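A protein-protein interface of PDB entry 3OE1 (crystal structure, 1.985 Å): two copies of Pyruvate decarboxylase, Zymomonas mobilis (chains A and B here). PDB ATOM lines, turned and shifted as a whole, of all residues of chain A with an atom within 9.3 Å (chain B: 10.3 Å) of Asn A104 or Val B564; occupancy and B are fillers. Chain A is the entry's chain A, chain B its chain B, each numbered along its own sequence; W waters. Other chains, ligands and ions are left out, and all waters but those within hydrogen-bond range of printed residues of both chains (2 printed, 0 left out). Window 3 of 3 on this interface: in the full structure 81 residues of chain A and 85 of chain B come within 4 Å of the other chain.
OD1 of Asp A105 lies within salt-bridge range of NH2 of Arg B561, at 2.8 Å.
The backbone NH (N) of Val B564 sits at hydrogen-bond distance from the side-chain amide oxygen (OD1) of Asn A104 (2.8 Å).
The side-chain amide nitrogen (ND2) of Asn A102 lies within hydrogen-bond range of the backbone carbonyl oxygen (O) of Asn B559 (2.7 Å).
ND2 of Asn A169 lies within hydrogen-bond range of O of Arg B561 (3.0 Å).
SG of Cys A168 is in hydrogen-bond range of O of Asn B559 (3.2 Å).
ND2 of Asn A102 sits at hydrogen-bond distance from O of Arg B561 (2.9 Å).
The side-chain amide nitrogen (ND2) of Asn A104 sits at hydrogen-bond distance from the backbone carbonyl oxygen (O) of Lys B562, 3.0 Å away.
OD1 of Asn A103 is in hydrogen-bond range of ND2 of Asn A169, 2.8 Å away.
O of Val B564 sits close to NZ of Lys B566, 3.5 Å away.
O of Ala A100 sits at hydrogen-bond distance from N of Cys A168 (2.9 Å).
ND2 of Asn A102 lies close to ND2 of Asn A169, at 3.4 Å.
The backbone NH (N) of Leu A112 is in hydrogen-bond range of the side-chain hydroxyl (OH) of Tyr A121.
O of His A110 is in hydrogen-bond range of OH of Tyr A121 (2.6 Å).
Among the printed residues, merely in contact across the chains: Asn A102 with Ala B558 (3.6 Å), Asn A103 with Pro B563 (3.5 Å), Asn A104 with Arg B561 (3.7 Å), Asn A104 with Pro B563 (3.7 Å), Asn A104 with Lys B566 (3.6 Å), His A110 with Trp B295 (3.9 Å), Leu A112 with Trp B295 (3.9 Å), Asn A169 with Asn B559 (3.6 Å), Asn A169 with Ser B560 (3.97 Å), Asn A169 with Lys B562 (3.98 Å), Asn A169 with Pro B563 (3.5 Å) and Met A173 with Pro B563 (3.7 Å).
Of the printed residues of chain B, Asn A103 touches Pro B563 (3.5 Å).
Asn A104 touches just these residues of chain B: Arg B561 (3.7 Å), Lys B562 (3.0 Å), Pro B563 (3.7 Å), Val B564 (2.8 Å) and Lys B566 (3.6 Å).
Tyr A121 touches none of the printed residues of chain B.
Of the printed residues of chain B, Cys A168 touches Asn B559 (3.2 Å).
Of the printed residues of chain A, Ala B558 touches Asn A102.
Of chain A, only Asn A103 (3.5 Å), Asn A104 (3.7 Å), Asn A169 (3.5 Å) and Met A173 (3.7 Å) come within 4 Å of Pro B563.
Printed residues of chain A within 4 Å of Val B564: Asn A104.
Printed residues of chain A within 4 Å of Lys B566: Asn A104.
The nearest residue of chain A that does not touch Val B564 is Asn A103 (4.9 Å).
Hydrophobic or aromatic side chains of chain A that line the printed part of chain B: His A110, Leu A112 and Met A173.
Hydrophobic or aromatic side chains of chain B that line the printed part of chain A: Trp B295, Pro B563 and Val B564.
No position is printed for both chains.
Of the 19 pairs that touch across the chains among the printed residues, none has its exchanged pair printed and touching as well.
Water W2 lies within hydrogen-bond range of OD2 of Asp A105 (2.7 Å), NH1 of Arg B561 (2.8 Å) and NE1 of Trp B295 (2.9 Å).
Water W1 lies within hydrogen-bond range of the guanidinium group (NE) of Arg B561 (3.1 Å) and the side-chain amide nitrogen (ND2) of Asn A104 (3.5 Å).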
ATOM      1  N   ALA A 100       0.865  31.487  24.668  1.00  0.00           N
ATOM      2  CA  ALA A 100       0.918  30.476  23.612  1.00  0.00           C
ATOM      3  C   ALA A 100       1.625  29.207  24.070  1.00  0.00           C
ATOM      4  O   ALA A 100       2.291  29.200  25.106  1.00  0.00           O
ATOM      5  CB  ALA A 100       1.591  31.051  22.357  1.00  0.00           C
ATOM      6  N   PRO A 101       1.468  28.118  23.303  1.00  0.00           N
ATOM      7  CA  PRO A 101       2.105  26.835  23.619  1.00  0.00           C
ATOM      8  C   PRO A 101       3.617  26.928  23.841  1.00  0.00           C
ATOM      9  O   PRO A 101       4.273  27.814  23.294  1.00  0.00           O
ATOM     10  CB  PRO A 101       1.825  26.002  22.371  1.00  0.00           C
ATOM     11  CG  PRO A 101       0.538  26.540  21.853  1.00  0.00           C
ATOM     12  CD  PRO A 101       0.544  28.010  22.158  1.00  0.00           C
ATOM     13  N   ASN A 102       4.140  26.008  24.649  1.00  0.00           N
ATOM     14  CA  ASN A 102       5.576  25.817  24.817  1.00  0.00           C
ATOM     15  C   ASN A 102       6.196  25.677  23.434  1.00  0.00           C
ATOM     16  O   ASN A 102       5.647  24.979  22.577  1.00  0.00           O
ATOM     17  CB  ASN A 102       5.833  24.555  25.648  1.00  0.00           C
ATOM     18  CG  ASN A 102       7.298  24.379  26.026  1.00  0.00           C
ATOM     19  OD1 ASN A 102       8.125  23.950  25.212  1.00  0.00           O
ATOM     20  ND2 ASN A 102       7.622  24.695  27.270  1.00  0.00           N
ATOM     21  N   ASN A 103       7.323  26.342  23.196  1.00  0.00           N
ATOM     22  CA  ASN A 103       7.877  26.352  21.844  1.00  0.00           C
ATOM     23  C   ASN A 103       8.353  24.981  21.348  1.00  0.00           C
ATOM     24  O   ASN A 103       8.507  24.773  20.149  1.00  0.00           O
ATOM     25  CB  ASN A 103       8.943  27.446  21.658  1.00  0.00           C
ATOM     26  CG  ASN A 103      10.241  27.163  22.406  1.00  0.00           C
ATOM     27  OD1 ASN A 103      10.332  26.254  23.232  1.00  0.00           O
ATOM     28  ND2 ASN A 103      11.256  27.973  22.121  1.00  0.00           N
ATOM     29  N   ASN A 104       8.552  24.045  22.271  1.00  0.00           N
ATOM     30  CA  ASN A 104       8.955  22.684  21.919  1.00  0.00           C
ATOM     31  C   ASN A 104       7.817  21.847  21.324  1.00  0.00           C
ATOM     32  O   ASN A 104       8.051  20.770  20.778  1.00  0.00           O
ATOM     33  CB  ASN A 104       9.527  21.959  23.144  1.00  0.00           C
ATOM     34  CG  ASN A 104      10.794  22.606  23.677  1.00  0.00           C
ATOM     35  OD1 ASN A 104      11.745  22.853  22.932  1.00  0.00           O
ATOM     36  ND2 ASN A 104      10.813  22.879  24.981  1.00  0.00           N
ATOM     37  N   ASP A 105       6.589  22.341  21.438  1.00  0.00           N
ATOM     38  CA  ASP A 105       5.412  21.589  20.998  1.00  0.00           C
ATOM     39  C   ASP A 105       5.040  21.777  19.532  1.00  0.00           C
ATOM     40  O   ASP A 105       4.023  21.254  19.078  1.00  0.00           O
ATOM     41  CB  ASP A 105       4.211  21.939  21.874  1.00  0.00           C
ATOM     42  CG  ASP A 105       4.366  21.431  23.278  1.00  0.00           C
ATOM     43  OD1 ASP A 105       4.877  20.306  23.433  1.00  0.00           O
ATOM     44  OD2 ASP A 105       3.998  22.157  24.221  1.00  0.00           O
ATOM     45  N   HIS A 106       5.855  22.526  18.798  1.00  0.00           N
ATOM     46  CA  HIS A 106       5.608  22.763  17.383  1.00  0.00           C
ATOM     47  C   HIS A 106       6.353  21.729  16.556  1.00  0.00           C
ATOM     48  O   HIS A 106       7.500  21.410  16.854  1.00  0.00           O
ATOM     49  CB  HIS A 106       6.067  24.167  16.988  1.00  0.00           C
ATOM     50  CG  HIS A 106       5.302  25.264  17.663  1.00  0.00           C
ATOM     51  ND1 HIS A 106       4.193  25.856  17.097  1.00  0.00           N
ATOM     52  CD2 HIS A 106       5.487  25.876  18.855  1.00  0.00           C
ATOM     53  CE1 HIS A 106       3.726  26.782  17.915  1.00  0.00           C
ATOM     54  NE2 HIS A 106       4.495  26.817  18.988  1.00  0.00           N
ATOM     55  N   ALA A 107       5.698  21.214  15.517  1.00  0.00           N
ATOM     56  CA  ALA A 107       6.283  20.186  14.663  1.00  0.00           C
ATOM     57  C   ALA A 107       6.752  18.996  15.499  1.00  0.00           C
ATOM     58  O   ALA A 107       7.817  18.420  15.256  1.00  0.00           O
ATOM     59  CB  ALA A 107       7.428  20.770  13.834  1.00  0.00           C
ATOM     60  N   ALA A 108       5.935  18.623  16.482  1.00  0.00           N
ATOM     61  CA  ALA A 108       6.302  17.574  17.425  1.00  0.00           C
ATOM     62  C   ALA A 108       5.251  16.471  17.510  1.00  0.00           C
ATOM     63  O   ALA A 108       5.463  15.461  18.171  1.00  0.00           O
ATOM     64  CB  ALA A 108       6.549  18.174  18.804  1.00  0.00           C
ATOM     65  N   GLY A 109       4.124  16.663  16.833  1.00  0.00           N
ATOM     66  CA  GLY A 109       3.032  15.711  16.904  1.00  0.00           C
ATOM     67  C   GLY A 109       2.343  15.749  18.256  1.00  0.00           C
ATOM     68  O   GLY A 109       1.746  14.764  18.687  1.00  0.00           O
ATOM     69  N   HIS A 110       2.439  16.892  18.928  1.00  0.00           N
ATOM     70  CA  HIS A 110       1.848  17.067  20.250  1.00  0.00           C
ATOM     71  C   HIS A 110       0.485  17.739  20.160  1.00  0.00           C
ATOM     72  O   HIS A 110       0.349  18.818  19.580  1.00  0.00           O
ATOM     73  CB  HIS A 110       2.761  17.909  21.142  1.00  0.00           C
ATOM     74  CG  HIS A 110       4.000  17.199  21.594  1.00  0.00           C
ATOM     75  ND1 HIS A 110       5.024  17.840  22.255  1.00  0.00           N
ATOM     76  CD2 HIS A 110       4.378  15.904  21.481  1.00  0.00           C
ATOM     77  CE1 HIS A 110       5.981  16.972  22.528  1.00  0.00           C
ATOM     78  NE2 HIS A 110       5.612  15.788  22.073  1.00  0.00           N
ATOM     79  N   LEU A 112      -2.356  19.609  22.292  1.00  0.00           N
ATOM     80  CA  LEU A 112      -2.314  20.405  23.517  1.00  0.00           C
ATOM     81  C   LEU A 112      -3.689  20.872  23.980  1.00  0.00           C
ATOM     82  O   LEU A 112      -4.618  20.958  23.193  1.00  0.00           O
ATOM     83  CB  LEU A 112      -1.412  21.618  23.327  1.00  0.00           C
ATOM     84  CG  LEU A 112       0.065  21.327  23.077  1.00  0.00           C
ATOM     85  CD1 LEU A 112       0.772  22.580  22.629  1.00  0.00           C
ATOM     86  CD2 LEU A 112       0.717  20.748  24.346  1.00  0.00           C
ATOM     87  N   THR A 119      -2.288  18.907  15.841  1.00  0.00           N
ATOM     88  CA  THR A 119      -0.923  19.095  16.328  1.00  0.00           C
ATOM     89  C   THR A 119      -0.217  20.335  15.771  1.00  0.00           C
ATOM     90  O   THR A 119       1.003  20.444  15.851  1.00  0.00           O
ATOM     91  CB  THR A 119      -0.055  17.848  16.060  1.00  0.00           C
ATOM     92  OG1 THR A 119       0.102  17.672  14.646  1.00  0.00           O
ATOM     93  CG2 THR A 119      -0.707  16.608  16.667  1.00  0.00           C
ATOM     94  N   TYR A 121      -0.363  24.803  15.606  1.00  0.00           N
ATOM     95  CA  TYR A 121      -0.845  25.909  16.417  1.00  0.00           C
ATOM     96  C   TYR A 121      -0.675  27.277  15.773  1.00  0.00           C
ATOM     97  O   TYR A 121      -0.417  28.262  16.448  1.00  0.00           O
ATOM     98  CB  TYR A 121      -0.186  25.835  17.792  1.00  0.00           C
ATOM     99  CG  TYR A 121      -0.452  24.487  18.414  1.00  0.00           C
ATOM    100  CD1 TYR A 121      -1.647  24.239  19.070  1.00  0.00           C
ATOM    101  CD2 TYR A 121       0.460  23.445  18.290  1.00  0.00           C
ATOM    102  CE1 TYR A 121      -1.916  23.004  19.618  1.00  0.00           C
ATOM    103  CE2 TYR A 121       0.200  22.195  18.838  1.00  0.00           C
ATOM    104  CZ  TYR A 121      -0.997  21.984  19.499  1.00  0.00           C
ATOM    105  OH  TYR A 121      -1.278  20.759  20.053  1.00  0.00           O
ATOM    106  N   TYR A 139       8.217  33.004  19.213  1.00  0.00           N
ATOM    107  CA  TYR A 139       8.558  31.632  19.569  1.00  0.00           C
ATOM    108  C   TYR A 139       9.912  31.523  20.280  1.00  0.00           C
ATOM    109  O   TYR A 139      10.160  30.557  21.003  1.00  0.00           O
ATOM    110  CB  TYR A 139       8.533  30.738  18.321  1.00  0.00           C
ATOM    111  CG  TYR A 139       7.162  30.614  17.686  1.00  0.00           C
ATOM    112  CD1 TYR A 139       6.043  30.330  18.459  1.00  0.00           C
ATOM    113  CD2 TYR A 139       6.986  30.787  16.319  1.00  0.00           C
ATOM    114  CE1 TYR A 139       4.786  30.219  17.890  1.00  0.00           C
ATOM    115  CE2 TYR A 139       5.721  30.678  15.735  1.00  0.00           C
ATOM    116  CZ  TYR A 139       4.627  30.392  16.531  1.00  0.00           C
ATOM    117  OH  TYR A 139       3.369  30.280  15.983  1.00  0.00           O
ATOM    118  N   THR A 140      10.789  32.504  20.063  1.00  0.00           N
ATOM    119  CA  THR A 140      12.072  32.550  20.763  1.00  0.00           C
ATOM    120  C   THR A 140      12.325  33.935  21.364  1.00  0.00           C
ATOM    121  O   THR A 140      11.763  34.939  20.904  1.00  0.00           O
ATOM    122  CB  THR A 140      13.264  32.180  19.840  1.00  0.00           C
ATOM    123  OG1 THR A 140      13.332  33.103  18.741  1.00  0.00           O
ATOM    124  CG2 THR A 140      13.119  30.764  19.317  1.00  0.00           C
ATOM    125  N   ALA A 167       5.155  32.369  23.311  1.00  0.00           N
ATOM    126  CA  ALA A 167       5.310  31.008  23.812  1.00  0.00           C
ATOM    127  C   ALA A 167       5.510  31.078  25.317  1.00  0.00           C
ATOM    128  O   ALA A 167       6.310  31.876  25.810  1.00  0.00           O
ATOM    129  CB  ALA A 167       6.480  30.316  23.139  1.00  0.00           C
ATOM    130  N   CYS A 168       4.772  30.251  26.046  1.00  0.00           N
ATOM    131  CA  CYS A 168       4.669  30.418  27.493  1.00  0.00           C
ATOM    132  C   CYS A 168       6.001  30.216  28.215  1.00  0.00           C
ATOM    133  O   CYS A 168       6.187  30.703  29.330  1.00  0.00           O
ATOM    134  CB  CYS A 168       3.599  29.488  28.067  1.00  0.00           C
ATOM    135  SG  CYS A 168       3.918  27.733  27.818  1.00  0.00           S
ATOM    136  N   ASN A 169       6.925  29.512  27.570  1.00  0.00           N
ATOM    137  CA  ASN A 169       8.205  29.185  28.191  1.00  0.00           C
ATOM    138  C   ASN A 169       9.324  30.176  27.889  1.00  0.00           C
ATOM    139  O   ASN A 169      10.462  29.963  28.294  1.00  0.00           O
ATOM    140  CB  ASN A 169       8.651  27.771  27.801  1.00  0.00           C
ATOM    141  CG  ASN A 169       8.893  27.623  26.309  1.00  0.00           C
ATOM    142  OD1 ASN A 169       8.207  28.237  25.487  1.00  0.00           O
ATOM    143  ND2 ASN A 169       9.867  26.805  25.952  1.00  0.00           N
ATOM    144  N   ILE A 170       9.012  31.255  27.177  1.00  0.00           N
ATOM    145  CA  ILE A 170      10.033  32.262  26.901  1.00  0.00           C
ATOM    146  C   ILE A 170       9.766  33.608  27.572  1.00  0.00           C
ATOM    147  O   ILE A 170      10.582  34.519  27.477  1.00  0.00           O
ATOM    148  CB  ILE A 170      10.240  32.481  25.399  1.00  0.00           C
ATOM    149  CG1 ILE A 170       9.019  33.172  24.790  1.00  0.00           C
ATOM    150  CG2 ILE A 170      10.547  31.157  24.710  1.00  0.00           C
ATOM    151  CD1 ILE A 170       9.245  33.636  23.376  1.00  0.00           C
ATOM    152  N   MET A 173      12.588  34.716  29.680  1.00  0.00           N
ATOM    153  CA  MET A 173      13.918  34.544  29.094  1.00  0.00           C
ATOM    154  C   MET A 173      14.558  35.868  28.688  1.00  0.00           C
ATOM    155  O   MET A 173      13.884  36.765  28.198  1.00  0.00           O
ATOM    156  CB  MET A 173      13.872  33.576  27.909  1.00  0.00           C
ATOM    157  CG  MET A 173      13.357  32.190  28.286  1.00  0.00           C
ATOM    158  SD  MET A 173      13.903  30.893  27.162  1.00  0.00           S
ATOM    159  CE  MET A 173      15.662  31.224  27.149  1.00  0.00           C
ATOM    160  N   TRP B 295       2.789  15.092  30.354  1.00  0.00           N
ATOM    161  CA  TRP B 295       3.620  14.229  29.524  1.00  0.00           C
ATOM    162  C   TRP B 295       4.371  13.188  30.347  1.00  0.00           C
ATOM    163  O   TRP B 295       5.358  12.618  29.882  1.00  0.00           O
ATOM    164  CB  TRP B 295       4.612  15.047  28.686  1.00  0.00           C
ATOM    165  CG  TRP B 295       3.981  16.037  27.738  1.00  0.00           C
ATOM    166  CD1 TRP B 295       4.149  17.393  27.739  1.00  0.00           C
ATOM    167  CD2 TRP B 295       3.100  15.745  26.642  1.00  0.00           C
ATOM    168  NE1 TRP B 295       3.427  17.962  26.717  1.00  0.00           N
ATOM    169  CE2 TRP B 295       2.776  16.974  26.027  1.00  0.00           C
ATOM    170  CE3 TRP B 295       2.556  14.564  26.120  1.00  0.00           C
ATOM    171  CZ2 TRP B 295       1.926  17.057  24.924  1.00  0.00           C
ATOM    172  CZ3 TRP B 295       1.720  14.647  25.026  1.00  0.00           C
ATOM    173  CH2 TRP B 295       1.413  15.887  24.437  1.00  0.00           C
ATOM    174  N   ALA B 557       5.287  22.233  35.216  1.00  0.00           N
ATOM    175  CA  ALA B 557       6.626  21.851  34.794  1.00  0.00           C
ATOM    176  C   ALA B 557       6.662  21.670  33.281  1.00  0.00           C
ATOM    177  O   ALA B 557       7.590  22.135  32.612  1.00  0.00           O
ATOM    178  CB  ALA B 557       7.085  20.577  35.510  1.00  0.00           C
ATOM    179  N   ALA B 558       5.641  21.008  32.746  1.00  0.00           N
ATOM    180  CA  ALA B 558       5.531  20.801  31.306  1.00  0.00           C
ATOM    181  C   ALA B 558       5.519  22.130  30.564  1.00  0.00           C
ATOM    182  O   ALA B 558       6.295  22.341  29.629  1.00  0.00           O
ATOM    183  CB  ALA B 558       4.278  20.006  30.977  1.00  0.00           C
ATOM    184  N   ASN B 559       4.631  23.024  30.993  1.00  0.00           N
ATOM    185  CA  ASN B 559       4.453  24.320  30.348  1.00  0.00           C
ATOM    186  C   ASN B 559       5.746  25.129  30.266  1.00  0.00           C
ATOM    187  O   ASN B 559       6.037  25.749  29.245  1.00  0.00           O
ATOM    188  CB  ASN B 559       3.380  25.144  31.075  1.00  0.00           C
ATOM    189  CG  ASN B 559       1.979  24.564  30.920  1.00  0.00           C
ATOM    190  OD1 ASN B 559       1.725  23.745  30.038  1.00  0.00           O
ATOM    191  ND2 ASN B 559       1.061  25.002  31.771  1.00  0.00           N
ATOM    192  N   SER B 560       6.526  25.118  31.342  1.00  0.00           N
ATOM    193  CA  SER B 560       7.643  26.043  31.454  1.00  0.00           C
ATOM    194  C   SER B 560       8.964  25.429  31.035  1.00  0.00           C
ATOM    195  O   SER B 560      10.004  26.078  31.123  1.00  0.00           O
ATOM    196  CB  SER B 560       7.758  26.571  32.882  1.00  0.00           C
ATOM    197  OG  SER B 560       8.028  25.520  33.789  1.00  0.00           O
ATOM    198  N   ARG B 561       8.934  24.182  30.580  1.00  0.00           N
ATOM    199  CA  ARG B 561      10.178  23.520  30.212  1.00  0.00           C
ATOM    200  C   ARG B 561      10.918  24.331  29.147  1.00  0.00           C
ATOM    201  O   ARG B 561      10.309  24.865  28.218  1.00  0.00           O
ATOM    202  CB  ARG B 561       9.942  22.069  29.785  1.00  0.00           C
ATOM    203  CG  ARG B 561       9.315  21.875  28.419  1.00  0.00           C
ATOM    204  CD  ARG B 561       9.007  20.398  28.197  1.00  0.00           C
ATOM    205  NE  ARG B 561       8.602  20.101  26.825  1.00  0.00           N
ATOM    206  CZ  ARG B 561       7.362  20.245  26.375  1.00  0.00           C
ATOM    207  NH1 ARG B 561       6.416  20.692  27.188  1.00  0.00           N
ATOM    208  NH2 ARG B 561       7.066  19.945  25.116  1.00  0.00           N
ATOM    209  N   LYS B 562      12.230  24.443  29.317  1.00  0.00           N
ATOM    210  CA  LYS B 562      13.053  25.326  28.499  1.00  0.00           C
ATOM    211  C   LYS B 562      13.175  24.873  27.038  1.00  0.00           C
ATOM    212  O   LYS B 562      13.108  23.676  26.739  1.00  0.00           O
ATOM    213  CB  LYS B 562      14.446  25.483  29.126  1.00  0.00           C
ATOM    214  CG  LYS B 562      14.486  26.383  30.363  1.00  0.00           C
ATOM    215  CD  LYS B 562      14.265  27.840  29.988  1.00  0.00           C
ATOM    216  CE  LYS B 562      14.286  28.750  31.208  1.00  0.00           C
ATOM    217  NZ  LYS B 562      15.663  28.923  31.751  1.00  0.00           N
ATOM    218  N   PRO B 563      13.348  25.839  26.121  1.00  0.00           N
ATOM    219  CA  PRO B 563      13.546  25.520  24.705  1.00  0.00           C
ATOM    220  C   PRO B 563      14.645  24.483  24.532  1.00  0.00           C
ATOM    221  O   PRO B 563      15.683  24.563  25.195  1.00  0.00           O
ATOM    222  CB  PRO B 563      13.987  26.857  24.111  1.00  0.00           C
ATOM    223  CG  PRO B 563      13.330  27.875  24.971  1.00  0.00           C
ATOM    224  CD  PRO B 563      13.315  27.293  26.360  1.00  0.00           C
ATOM    225  N   VAL B 564      14.413  23.515  23.652  1.00  0.00           N
ATOM    226  CA  VAL B 564      15.423  22.515  23.338  1.00  0.00           C
ATOM    227  C   VAL B 564      16.198  22.952  22.097  1.00  0.00           C
ATOM    228  O   VAL B 564      15.613  23.193  21.041  1.00  0.00           O
ATOM    229  CB  VAL B 564      14.794  21.132  23.104  1.00  0.00           C
ATOM    230  CG1 VAL B 564      15.873  20.088  22.918  1.00  0.00           C
ATOM    231  CG2 VAL B 564      13.885  20.757  24.267  1.00  0.00           C
ATOM    232  N   ASN B 565      17.516  23.053  22.231  1.00  0.00           N
ATOM    233  CA  ASN B 565      18.366  23.561  21.154  1.00  0.00           C
ATOM    234  C   ASN B 565      18.069  22.927  19.798  1.00  0.00           C
ATOM    235  O   ASN B 565      18.122  21.709  19.647  1.00  0.00           O
ATOM    236  CB  ASN B 565      19.839  23.385  21.514  1.00  0.00           C
ATOM    237  CG  ASN B 565      20.152  23.886  22.908  1.00  0.00           C
ATOM    238  OD1 ASN B 565      20.339  25.085  23.123  1.00  0.00           O
ATOM    239  ND2 ASN B 565      20.203  22.970  23.869  1.00  0.00           N
ATOM    240  N   LYS B 566      17.754  23.764  18.815  1.00  0.00           N
ATOM    241  CA  LYS B 566      17.325  23.285  17.504  1.00  0.00           C
ATOM    242  C   LYS B 566      18.375  23.493  16.413  1.00  0.00           C
ATOM    243  O   LYS B 566      18.114  23.270  15.226  1.00  0.00           O
ATOM    244  CB  LYS B 566      15.999  23.939  17.112  1.00  0.00           C
ATOM    245  CG  LYS B 566      14.818  23.431  17.924  1.00  0.00           C
ATOM    246  CD  LYS B 566      13.525  24.126  17.545  1.00  0.00           C
ATOM    247  CE  LYS B 566      12.330  23.322  18.015  1.00  0.00           C
ATOM    248  NZ  LYS B 566      12.542  22.841  19.411  1.00  0.00           N
HETATM  249  O   HOH W   1      11.384  19.502  25.549  1.00  0.00           O
HETATM  250  O   HOH W   2       3.657  20.894  26.542  1.00  0.00           O
